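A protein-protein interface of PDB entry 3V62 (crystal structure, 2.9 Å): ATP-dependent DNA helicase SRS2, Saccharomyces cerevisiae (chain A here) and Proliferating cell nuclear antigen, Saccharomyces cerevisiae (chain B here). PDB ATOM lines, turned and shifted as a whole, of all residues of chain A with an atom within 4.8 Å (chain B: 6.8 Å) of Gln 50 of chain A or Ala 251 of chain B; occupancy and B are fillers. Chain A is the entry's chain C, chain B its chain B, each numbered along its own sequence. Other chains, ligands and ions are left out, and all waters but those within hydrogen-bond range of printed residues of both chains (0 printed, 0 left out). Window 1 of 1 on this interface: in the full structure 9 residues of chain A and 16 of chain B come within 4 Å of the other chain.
Among the printed residues, pairs that only touch across the chains: Met 45 of chain A with Pro 252 of chain B (3.2 Å), Phe 48 of chain A with Arg 44 of chain B (3.3 Å), Gln 50 of chain A with Ala 251 of chain B (3.3 Å), Gln 50 of chain A with Pro 234 of chain B (3.3 Å), Ile 47 of chain A with Phe 249 of chain B (3.4 Å), Ile 47 of chain A with Val 45 of chain B (3.5 Å), Gln 50 of chain A with Pro 252 of chain B (3.5 Å), Gln 44 of chain A with Lys 253 of chain B (3.5 Å), Ile 47 of chain A with Pro 234 of chain B (3.6 Å), Met 45 of chain A with Ala 251 of chain B (3.7 Å), Ile 47 of chain A with Leu 47 of chain B (3.8 Å), Ile 47 of chain A with Ala 251 of chain B (3.8 Å), Gln 44 of chain A with Val 45 of chain B (3.8 Å), Gln 44 of chain A with Tyr 211 of chain B (3.9 Å), Met 45 of chain A with Lys 253 of chain B (3.9 Å) and Met 45 of chain A with Val 45 of chain B (3.9 Å).
Gln 50 of chain A touches five residues of chain B.
Ala 251 of chain B touches just these residues of chain A: Gln 44, Met 45, Ile 47 and Gln 50.
Printed residues of chain A within 4 Å of Pro 234 of chain B: Ile 47 (3.6 Å) and Gln 50 (3.3 Å).
Of the printed residues of chain A, Arg 44 of chain B touches Asp 46 (3.0 Å), Ile 47 (3.1 Å) and Phe 48 (3.3 Å).
Of the printed residues of chain B, Phe 48 of chain A touches Arg 44 (3.3 Å).
Of the printed residues of chain A, Tyr 211 of chain B touches Gln 44.
Printed residues of chain A within 4 Å of Lys 253 of chain B: Gln 44 and Met 45.
Leu 205 of chain B touches none of the printed residues of chain A.
Phe 207 of chain B touches none of the printed residues of chain A.
The nearest printed residue of chain B that does not touch Phe 48 of chain A is Leu 47 of chain B (4.2 Å).
N of Ala 251 of chain B sits at hydrogen-bond distance from O of Val 45 of chain B, at 3.4 Å.
O of Leu 47 of chain B sits at hydrogen-bond distance from N of Phe 249 of chain B (2.8 Å).
The backbone NH (N) of Lys 253 of chain B is in hydrogen-bond range of the backbone carbonyl oxygen (O) of Thr 206 of chain B (2.8 Å).
The side-chain carboxylate (OD2) of Asp 46 of chain A sits close to the backbone NH (N) of Phe 48 of chain A (3.4 Å).
OD2 of Asp 46 of chain A is in hydrogen-bond range of N of Ser 49 of chain A (2.8 Å).
The backbone carbonyl oxygen (O) of Phe 48 of chain A sits at hydrogen-bond distance from the side-chain hydroxyl (OG) of Ser 52 of chain A, 3.4 Å away.
The backbone carbonyl oxygen (O) of Arg 44 of chain B lies close to the backbone NH (N) of Ile 47 of chain A (3.1 Å).
OE2 of Glu 232 of chain B is in hydrogen-bond range of NE2 of Gln 50 of chain A.
NE2 of Gln 50 of chain A sits close to N of Ala 233 of chain B, 3.2 Å away.
O of Ala 251 of chain B lies within hydrogen-bond range of NE2 of Gln 44 of chain A (2.7 Å).
The side-chain amide nitrogen (NE2) of Gln 44 of chain A lies within hydrogen-bond range of the backbone carbonyl oxygen (O) of Pro 252 of chain B, 3.4 Å away.
SD of Met 45 of chain A lies close to OE2 of Glu 232 of chain B, at 3.7 Å.
OD1 of Asp 46 of chain A lies close to O of Arg 44 of chain B, at 3.0 Å.
Hydrophobic or aromatic side chains of chain A within 4 Å of the printed part of chain B: Met 45, Ile 47 and Phe 48.
Of the 21 printed residues of chain B, 11 touch a printed residue of chain A.
Printed residues of chain B that touch a printed residue of chain A: Arg 44, Val 45, Leu 47, Tyr 211, Glu 232, Ala 233, Pro 234, Phe 249, Ala 251, Pro 252 and Lys 253.
Hydrophobic or aromatic side chains of chain B within 4 Å of the printed part of chain A: Val 45, Leu 47, Tyr 211, Pro 234, Ala 251 and Pro 252.
Among the printed residues, 23 pairs touch across the chains.
Among the printed residues, no Asp or Glu carboxylate lies within 4 Å of a Lys or Arg side-chain nitrogen of the other chain.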
ATOM      1  N   GLN A  44      10.668  13.275  21.733  1.00  0.00           N
ATOM      2  CA  GLN A  44       9.851  12.420  20.857  1.00  0.00           C
ATOM      3  C   GLN A  44       9.367  13.163  19.614  1.00  0.00           C
ATOM      4  O   GLN A  44       9.103  14.366  19.666  1.00  0.00           O
ATOM      5  CB  GLN A  44       8.652  11.847  21.633  1.00  0.00           C
ATOM      6  CG  GLN A  44       7.791  10.839  20.874  1.00  0.00           C
ATOM      7  CD  GLN A  44       8.447   9.471  20.708  1.00  0.00           C
ATOM      8  OE1 GLN A  44       8.691   8.751  21.685  1.00  0.00           O
ATOM      9  NE2 GLN A  44       8.719   9.097  19.460  1.00  0.00           N
ATOM     10  N   MET A  45       9.255  12.446  18.499  1.00  0.00           N
ATOM     11  CA  MET A  45       8.725  13.036  17.274  1.00  0.00           C
ATOM     12  C   MET A  45       7.359  12.447  16.881  1.00  0.00           C
ATOM     13  O   MET A  45       7.006  11.346  17.306  1.00  0.00           O
ATOM     14  CB  MET A  45       9.752  12.957  16.134  1.00  0.00           C
ATOM     15  CG  MET A  45      10.018  11.568  15.584  1.00  0.00           C
ATOM     16  SD  MET A  45      11.361  11.579  14.381  1.00  0.00           S
ATOM     17  CE  MET A  45      12.764  11.116  15.396  1.00  0.00           C
ATOM     18  N   ASP A  46       6.600  13.209  16.091  1.00  0.00           N
ATOM     19  CA  ASP A  46       5.265  12.821  15.617  1.00  0.00           C
ATOM     20  C   ASP A  46       5.346  11.789  14.482  1.00  0.00           C
ATOM     21  O   ASP A  46       6.172  11.921  13.571  1.00  0.00           O
ATOM     22  CB  ASP A  46       4.491  14.076  15.182  1.00  0.00           C
ATOM     23  CG  ASP A  46       3.292  13.764  14.300  1.00  0.00           C
ATOM     24  OD1 ASP A  46       2.382  13.042  14.756  1.00  0.00           O
ATOM     25  OD2 ASP A  46       3.251  14.257  13.150  1.00  0.00           O
ATOM     26  N   ILE A  47       4.484  10.771  14.546  1.00  0.00           N
ATOM     27  CA  ILE A  47       4.517   9.629  13.615  1.00  0.00           C
ATOM     28  C   ILE A  47       4.213  10.010  12.163  1.00  0.00           C
ATOM     29  O   ILE A  47       4.656   9.336  11.229  1.00  0.00           O
ATOM     30  CB  ILE A  47       3.586   8.474  14.079  1.00  0.00           C
ATOM     31  CG1 ILE A  47       3.649   7.275  13.128  1.00  0.00           C
ATOM     32  CG2 ILE A  47       2.145   8.934  14.227  1.00  0.00           C
ATOM     33  CD1 ILE A  47       4.670   6.244  13.523  1.00  0.00           C
ATOM     34  N   PHE A  48       3.462  11.092  11.986  1.00  0.00           N
ATOM     35  CA  PHE A  48       3.065  11.547  10.665  1.00  0.00           C
ATOM     36  C   PHE A  48       4.086  12.497  10.046  1.00  0.00           C
ATOM     37  O   PHE A  48       4.412  12.367   8.865  1.00  0.00           O
ATOM     38  CB  PHE A  48       1.723  12.242  10.745  1.00  0.00           C
ATOM     39  CG  PHE A  48       0.608  11.352  11.158  1.00  0.00           C
ATOM     40  CD1 PHE A  48       0.036  11.487  12.414  1.00  0.00           C
ATOM     41  CD2 PHE A  48       0.108  10.391  10.286  1.00  0.00           C
ATOM     42  CE1 PHE A  48      -1.021  10.673  12.799  1.00  0.00           C
ATOM     43  CE2 PHE A  48      -0.952   9.575  10.664  1.00  0.00           C
ATOM     44  CZ  PHE A  48      -1.518   9.718  11.923  1.00  0.00           C
ATOM     45  N   SER A  49       4.575  13.457  10.837  1.00  0.00           N
ATOM     46  CA  SER A  49       5.624  14.366  10.375  1.00  0.00           C
ATOM     47  C   SER A  49       6.931  13.600  10.117  1.00  0.00           C
ATOM     48  O   SER A  49       7.865  14.122   9.499  1.00  0.00           O
ATOM     49  CB  SER A  49       5.815  15.560  11.334  1.00  0.00           C
ATOM     50  OG  SER A  49       6.221  15.151  12.624  1.00  0.00           O
ATOM     51  N   GLN A  50       6.970  12.349  10.576  1.00  0.00           N
ATOM     52  CA  GLN A  50       8.068  11.439  10.270  1.00  0.00           C
ATOM     53  C   GLN A  50       7.754  10.574   9.043  1.00  0.00           C
ATOM     54  O   GLN A  50       8.669  10.130   8.361  1.00  0.00           O
ATOM     55  CB  GLN A  50       8.407  10.562  11.480  1.00  0.00           C
ATOM     56  CG  GLN A  50       9.850  10.090  11.490  1.00  0.00           C
ATOM     57  CD  GLN A  50      10.031   8.748  12.169  1.00  0.00           C
ATOM     58  OE1 GLN A  50       9.124   8.249  12.831  1.00  0.00           O
ATOM     59  NE2 GLN A  50      11.209   8.150  12.003  1.00  0.00           N
ATOM     60  N   LEU A  51       6.472  10.330   8.773  1.00  0.00           N
ATOM     61  CA  LEU A  51       6.058   9.643   7.539  1.00  0.00           C
ATOM     62  C   LEU A  51       6.079  10.590   6.349  1.00  0.00           C
ATOM     63  O   LEU A  51       6.292  10.162   5.211  1.00  0.00           O
ATOM     64  CB  LEU A  51       4.675   9.006   7.681  1.00  0.00           C
ATOM     65  CG  LEU A  51       4.663   7.576   8.227  1.00  0.00           C
ATOM     66  CD1 LEU A  51       3.336   7.269   8.902  1.00  0.00           C
ATOM     67  CD2 LEU A  51       4.982   6.546   7.147  1.00  0.00           C
ATOM     68  N   SER A  52       5.851  11.873   6.631  1.00  0.00           N
ATOM     69  CA  SER A  52       5.962  12.939   5.638  1.00  0.00           C
ATOM     70  C   SER A  52       7.423  13.171   5.281  1.00  0.00           C
ATOM     71  O   SER A  52       7.819  12.959   4.131  1.00  0.00           O
ATOM     72  CB  SER A  52       5.325  14.234   6.141  1.00  0.00           C
ATOM     73  OG  SER A  52       3.918  14.185   6.010  1.00  0.00           O
ATOM     74  N   ARG A  53       8.221  13.582   6.265  1.00  0.00           N
ATOM     75  CA  ARG A  53       9.655  13.784   6.056  1.00  0.00           C
ATOM     76  C   ARG A  53      10.368  12.567   5.452  1.00  0.00           C
ATOM     77  O   ARG A  53      11.261  12.731   4.622  1.00  0.00           O
ATOM     78  CB  ARG A  53      10.344  14.251   7.339  1.00  0.00           C
ATOM     79  CG  ARG A  53      10.222  15.748   7.544  1.00  0.00           C
ATOM     80  CD  ARG A  53      10.926  16.220   8.799  1.00  0.00           C
ATOM     81  NE  ARG A  53      10.711  17.653   8.993  1.00  0.00           N
ATOM     82  CZ  ARG A  53      10.798  18.285  10.162  1.00  0.00           C
ATOM     83  NH1 ARG A  53      11.095  17.618  11.273  1.00  0.00           N
ATOM     84  NH2 ARG A  53      10.581  19.594  10.226  1.00  0.00           N
ATOM     85  N   ALA A  54       9.953  11.362   5.847  1.00  0.00           N
ATOM     86  CA  ALA A  54      10.542  10.112   5.342  1.00  0.00           C
ATOM     87  C   ALA A  54      10.256   9.886   3.864  1.00  0.00           C
ATOM     88  O   ALA A  54      11.177   9.638   3.076  1.00  0.00           O
ATOM     89  CB  ALA A  54      10.058   8.915   6.152  1.00  0.00           C
ATOM     90  N   ARG B  44      -0.234  10.613  19.235  1.00  0.00           N
ATOM     91  CA  ARG B  44       0.093  10.659  17.805  1.00  0.00           C
ATOM     92  C   ARG B  44       1.496  10.117  17.456  1.00  0.00           C
ATOM     93  O   ARG B  44       2.246  10.750  16.717  1.00  0.00           O
ATOM     94  CB  ARG B  44      -0.053  12.098  17.302  1.00  0.00           C
ATOM     95  CG  ARG B  44      -0.700  12.236  15.941  1.00  0.00           C
ATOM     96  CD  ARG B  44      -2.040  12.949  16.044  1.00  0.00           C
ATOM     97  NE  ARG B  44      -2.782  12.887  14.786  1.00  0.00           N
ATOM     98  CZ  ARG B  44      -2.433  13.527  13.667  1.00  0.00           C
ATOM     99  NH1 ARG B  44      -1.336  14.282  13.634  1.00  0.00           N
ATOM    100  NH2 ARG B  44      -3.174  13.396  12.568  1.00  0.00           N
ATOM    101  N   VAL B  45       1.831   8.930  17.954  1.00  0.00           N
ATOM    102  CA  VAL B  45       3.204   8.413  17.928  1.00  0.00           C
ATOM    103  C   VAL B  45       3.156   6.933  17.556  1.00  0.00           C
ATOM    104  O   VAL B  45       4.092   6.372  16.947  1.00  0.00           O
ATOM    105  CB  VAL B  45       3.853   8.578  19.335  1.00  0.00           C
ATOM    106  CG1 VAL B  45       5.114   7.746  19.487  1.00  0.00           C
ATOM    107  CG2 VAL B  45       4.136  10.042  19.662  1.00  0.00           C
ATOM    108  N   LEU B  46       2.053   6.296  17.946  1.00  0.00           N
ATOM    109  CA  LEU B  46       1.866   4.866  17.730  1.00  0.00           C
ATOM    110  C   LEU B  46       0.759   4.637  16.723  1.00  0.00           C
ATOM    111  O   LEU B  46      -0.207   5.390  16.656  1.00  0.00           O
ATOM    112  CB  LEU B  46       1.584   4.124  19.047  1.00  0.00           C
ATOM    113  CG  LEU B  46       1.738   2.587  19.032  1.00  0.00           C
ATOM    114  CD1 LEU B  46       2.955   2.066  18.270  1.00  0.00           C
ATOM    115  CD2 LEU B  46       1.772   2.020  20.440  1.00  0.00           C
ATOM    116  N   LEU B  47       0.919   3.597  15.928  1.00  0.00           N
ATOM    117  CA  LEU B  47      -0.009   3.304  14.883  1.00  0.00           C
ATOM    118  C   LEU B  47      -0.217   1.812  14.947  1.00  0.00           C
ATOM    119  O   LEU B  47       0.745   1.030  14.819  1.00  0.00           O
ATOM    120  CB  LEU B  47       0.631   3.652  13.563  1.00  0.00           C
ATOM    121  CG  LEU B  47      -0.041   4.601  12.593  1.00  0.00           C
ATOM    122  CD1 LEU B  47      -0.008   6.037  13.113  1.00  0.00           C
ATOM    123  CD2 LEU B  47       0.711   4.483  11.276  1.00  0.00           C
ATOM    124  N   LEU B 131       7.236   0.904   3.329  1.00  0.00           N
ATOM    125  CA  LEU B 131       8.586   1.435   3.123  1.00  0.00           C
ATOM    126  C   LEU B 131       9.554   0.277   2.930  1.00  0.00           C
ATOM    127  O   LEU B 131       9.141  -0.808   2.500  1.00  0.00           O
ATOM    128  CB  LEU B 131       8.993   2.329   4.302  1.00  0.00           C
ATOM    129  CG  LEU B 131       7.846   3.252   4.745  1.00  0.00           C
ATOM    130  CD1 LEU B 131       7.996   3.757   6.178  1.00  0.00           C
ATOM    131  CD2 LEU B 131       7.648   4.388   3.742  1.00  0.00           C
ATOM    132  N   LEU B 205      18.425   2.946  17.052  1.00  0.00           N
ATOM    133  CA  LEU B 205      17.310   3.808  17.426  1.00  0.00           C
ATOM    134  C   LEU B 205      16.920   3.757  18.912  1.00  0.00           C
ATOM    135  O   LEU B 205      17.280   2.838  19.641  1.00  0.00           O
ATOM    136  CB  LEU B 205      16.104   3.450  16.583  1.00  0.00           C
ATOM    137  CG  LEU B 205      16.310   3.614  15.096  1.00  0.00           C
ATOM    138  CD1 LEU B 205      15.881   2.325  14.428  1.00  0.00           C
ATOM    139  CD2 LEU B 205      15.546   4.816  14.562  1.00  0.00           C
ATOM    140  N   THR B 206      16.153   4.757  19.334  1.00  0.00           N
ATOM    141  CA  THR B 206      15.654   4.858  20.696  1.00  0.00           C
ATOM    142  C   THR B 206      14.145   5.111  20.711  1.00  0.00           C
ATOM    143  O   THR B 206      13.637   5.986  19.999  1.00  0.00           O
ATOM    144  CB  THR B 206      16.390   5.983  21.452  1.00  0.00           C
ATOM    145  OG1 THR B 206      17.778   5.643  21.567  1.00  0.00           O
ATOM    146  CG2 THR B 206      15.810   6.196  22.837  1.00  0.00           C
ATOM    147  N   PHE B 207      13.446   4.350  21.551  1.00  0.00           N
ATOM    148  CA  PHE B 207      12.006   4.441  21.689  1.00  0.00           C
ATOM    149  C   PHE B 207      11.546   4.681  23.118  1.00  0.00           C
ATOM    150  O   PHE B 207      12.137   4.146  24.051  1.00  0.00           O
ATOM    151  CB  PHE B 207      11.402   3.143  21.201  1.00  0.00           C
ATOM    152  CG  PHE B 207      11.789   2.801  19.801  1.00  0.00           C
ATOM    153  CD1 PHE B 207      11.215   3.476  18.728  1.00  0.00           C
ATOM    154  CD2 PHE B 207      12.725   1.810  19.553  1.00  0.00           C
ATOM    155  CE1 PHE B 207      11.571   3.168  17.429  1.00  0.00           C
ATOM    156  CE2 PHE B 207      13.080   1.489  18.254  1.00  0.00           C
ATOM    157  CZ  PHE B 207      12.507   2.172  17.190  1.00  0.00           C
ATOM    158  N   GLY B 208      10.483   5.476  23.272  1.00  0.00           N
ATOM    159  CA  GLY B 208       9.749   5.583  24.543  1.00  0.00           C
ATOM    160  C   GLY B 208       9.299   4.212  25.040  1.00  0.00           C
ATOM    161  O   GLY B 208       8.711   3.420  24.293  1.00  0.00           O
ATOM    162  N   TYR B 211       5.377   3.024  25.168  1.00  0.00           N
ATOM    163  CA  TYR B 211       4.843   2.521  23.914  1.00  0.00           C
ATOM    164  C   TYR B 211       5.278   1.094  23.701  1.00  0.00           C
ATOM    165  O   TYR B 211       4.492   0.256  23.274  1.00  0.00           O
ATOM    166  CB  TYR B 211       5.329   3.362  22.756  1.00  0.00           C
ATOM    167  CG  TYR B 211       5.086   4.821  22.948  1.00  0.00           C
ATOM    168  CD1 TYR B 211       3.868   5.389  22.594  1.00  0.00           C
ATOM    169  CD2 TYR B 211       6.077   5.648  23.476  1.00  0.00           C
ATOM    170  CE1 TYR B 211       3.641   6.744  22.762  1.00  0.00           C
ATOM    171  CE2 TYR B 211       5.856   7.009  23.648  1.00  0.00           C
ATOM    172  CZ  TYR B 211       4.634   7.543  23.288  1.00  0.00           C
ATOM    173  OH  TYR B 211       4.384   8.876  23.461  1.00  0.00           O
ATOM    174  N   SER B 230      14.625   1.059  10.462  1.00  0.00           N
ATOM    175  CA  SER B 230      15.363   1.741   9.437  1.00  0.00           C
ATOM    176  C   SER B 230      15.708   3.120   9.973  1.00  0.00           C
ATOM    177  O   SER B 230      14.953   3.674  10.767  1.00  0.00           O
ATOM    178  CB  SER B 230      14.534   1.778   8.153  1.00  0.00           C
ATOM    179  OG  SER B 230      14.365   3.096   7.690  1.00  0.00           O
ATOM    180  N   SER B 231      16.873   3.638   9.584  1.00  0.00           N
ATOM    181  CA  SER B 231      17.300   4.997   9.937  1.00  0.00           C
ATOM    182  C   SER B 231      16.285   6.026   9.461  1.00  0.00           C
ATOM    183  O   SER B 231      16.020   6.156   8.259  1.00  0.00           O
ATOM    184  CB  SER B 231      18.662   5.316   9.320  1.00  0.00           C
ATOM    185  OG  SER B 231      19.703   4.662  10.015  1.00  0.00           O
ATOM    186  N   GLU B 232      15.716   6.755  10.408  1.00  0.00           N
ATOM    187  CA  GLU B 232      14.634   7.691  10.106  1.00  0.00           C
ATOM    188  C   GLU B 232      13.484   7.105   9.248  1.00  0.00           C
ATOM    189  O   GLU B 232      13.311   7.420   8.062  1.00  0.00           O
ATOM    190  CB  GLU B 232      15.178   9.028   9.573  1.00  0.00           C
ATOM    191  CG  GLU B 232      15.622   9.973  10.688  1.00  0.00           C
ATOM    192  CD  GLU B 232      14.593  10.082  11.812  1.00  0.00           C
ATOM    193  OE1 GLU B 232      14.911   9.702  12.962  1.00  0.00           O
ATOM    194  OE2 GLU B 232      13.454  10.529  11.542  1.00  0.00           O
ATOM    195  N   ALA B 233      12.745   6.210   9.903  1.00  0.00           N
ATOM    196  CA  ALA B 233      11.475   5.632   9.469  1.00  0.00           C
ATOM    197  C   ALA B 233      10.910   5.024  10.753  1.00  0.00           C
ATOM    198  O   ALA B 233      11.673   4.548  11.616  1.00  0.00           O
ATOM    199  CB  ALA B 233      11.671   4.556   8.406  1.00  0.00           C
ATOM    200  N   PRO B 234       9.582   5.049  10.914  1.00  0.00           N
ATOM    201  CA  PRO B 234       9.050   4.378  12.091  1.00  0.00           C
ATOM    202  C   PRO B 234       9.343   2.863  12.089  1.00  0.00           C
ATOM    203  O   PRO B 234       9.291   2.210  11.037  1.00  0.00           O
ATOM    204  CB  PRO B 234       7.548   4.651  11.997  1.00  0.00           C
ATOM    205  CG  PRO B 234       7.434   5.885  11.173  1.00  0.00           C
ATOM    206  CD  PRO B 234       8.545   5.784  10.172  1.00  0.00           C
ATOM    207  N   ALA B 235       9.665   2.328  13.263  1.00  0.00           N
ATOM    208  CA  ALA B 235       9.919   0.905  13.420  1.00  0.00           C
ATOM    209  C   ALA B 235       8.646   0.103  13.253  1.00  0.00           C
ATOM    210  O   ALA B 235       7.569   0.530  13.648  1.00  0.00           O
ATOM    211  CB  ALA B 235      10.525   0.621  14.778  1.00  0.00           C
ATOM    212  N   PHE B 249       3.448   0.737  14.331  1.00  0.00           N
ATOM    213  CA  PHE B 249       4.446   1.606  13.757  1.00  0.00           C
ATOM    214  C   PHE B 249       4.754   2.626  14.808  1.00  0.00           C
ATOM    215  O   PHE B 249       3.882   3.385  15.233  1.00  0.00           O
ATOM    216  CB  PHE B 249       3.949   2.267  12.472  1.00  0.00           C
ATOM    217  CG  PHE B 249       3.572   1.286  11.384  1.00  0.00           C
ATOM    218  CD1 PHE B 249       2.276   0.773  11.297  1.00  0.00           C
ATOM    219  CD2 PHE B 249       4.506   0.880  10.444  1.00  0.00           C
ATOM    220  CE1 PHE B 249       1.935  -0.132  10.296  1.00  0.00           C
ATOM    221  CE2 PHE B 249       4.161  -0.017   9.438  1.00  0.00           C
ATOM    222  CZ  PHE B 249       2.880  -0.522   9.361  1.00  0.00           C
ATOM    223  N   LEU B 250       6.006   2.621  15.248  1.00  0.00           N
ATOM    224  CA  LEU B 250       6.427   3.452  16.363  1.00  0.00           C
ATOM    225  C   LEU B 250       7.516   4.375  15.923  1.00  0.00           C
ATOM    226  O   LEU B 250       8.510   3.927  15.346  1.00  0.00           O
ATOM    227  CB  LEU B 250       6.953   2.578  17.506  1.00  0.00           C
ATOM    228  CG  LEU B 250       7.371   3.334  18.768  1.00  0.00           C
ATOM    229  CD1 LEU B 250       6.258   4.238  19.293  1.00  0.00           C
ATOM    230  CD2 LEU B 250       7.842   2.371  19.842  1.00  0.00           C
ATOM    231  N   ALA B 251       7.332   5.657  16.213  1.00  0.00           N
ATOM    232  CA  ALA B 251       8.339   6.679  15.927  1.00  0.00           C
ATOM    233  C   ALA B 251       9.457   6.690  16.970  1.00  0.00           C
ATOM    234  O   ALA B 251       9.191   6.729  18.172  1.00  0.00           O
ATOM    235  CB  ALA B 251       7.689   8.056  15.840  1.00  0.00           C
ATOM    236  N   PRO B 252      10.718   6.669  16.511  1.00  0.00           N
ATOM    237  CA  PRO B 252      11.837   6.780  17.435  1.00  0.00           C
ATOM    238  C   PRO B 252      11.961   8.215  17.913  1.00  0.00           C
ATOM    239  O   PRO B 252      11.324   9.087  17.339  1.00  0.00           O
ATOM    240  CB  PRO B 252      13.034   6.381  16.571  1.00  0.00           C
ATOM    241  CG  PRO B 252      12.644   6.768  15.188  1.00  0.00           C
ATOM    242  CD  PRO B 252      11.163   6.567  15.110  1.00  0.00           C
ATOM    243  N   LYS B 253      12.748   8.460  18.958  1.00  0.00           N
ATOM    244  CA  LYS B 253      12.977   9.836  19.424  1.00  0.00           C
ATOM    245  C   LYS B 253      14.295  10.406  18.887  1.00  0.00           C
ATOM    246  O   LYS B 253      15.282   9.682  18.791  1.00  0.00           O
ATOM    247  CB  LYS B 253      12.897   9.929  20.948  1.00  0.00           C
ATOM    248  CG  LYS B 253      13.254   8.644  21.668  1.00  0.00           C
ATOM    249  CD  LYS B 253      13.090   8.783  23.173  1.00  0.00           C
ATOM    250  CE  LYS B 253      11.639   8.733  23.616  1.00  0.00           C
ATOM    251  NZ  LYS B 253      11.569   8.768  25.103  1.00  0.00           N
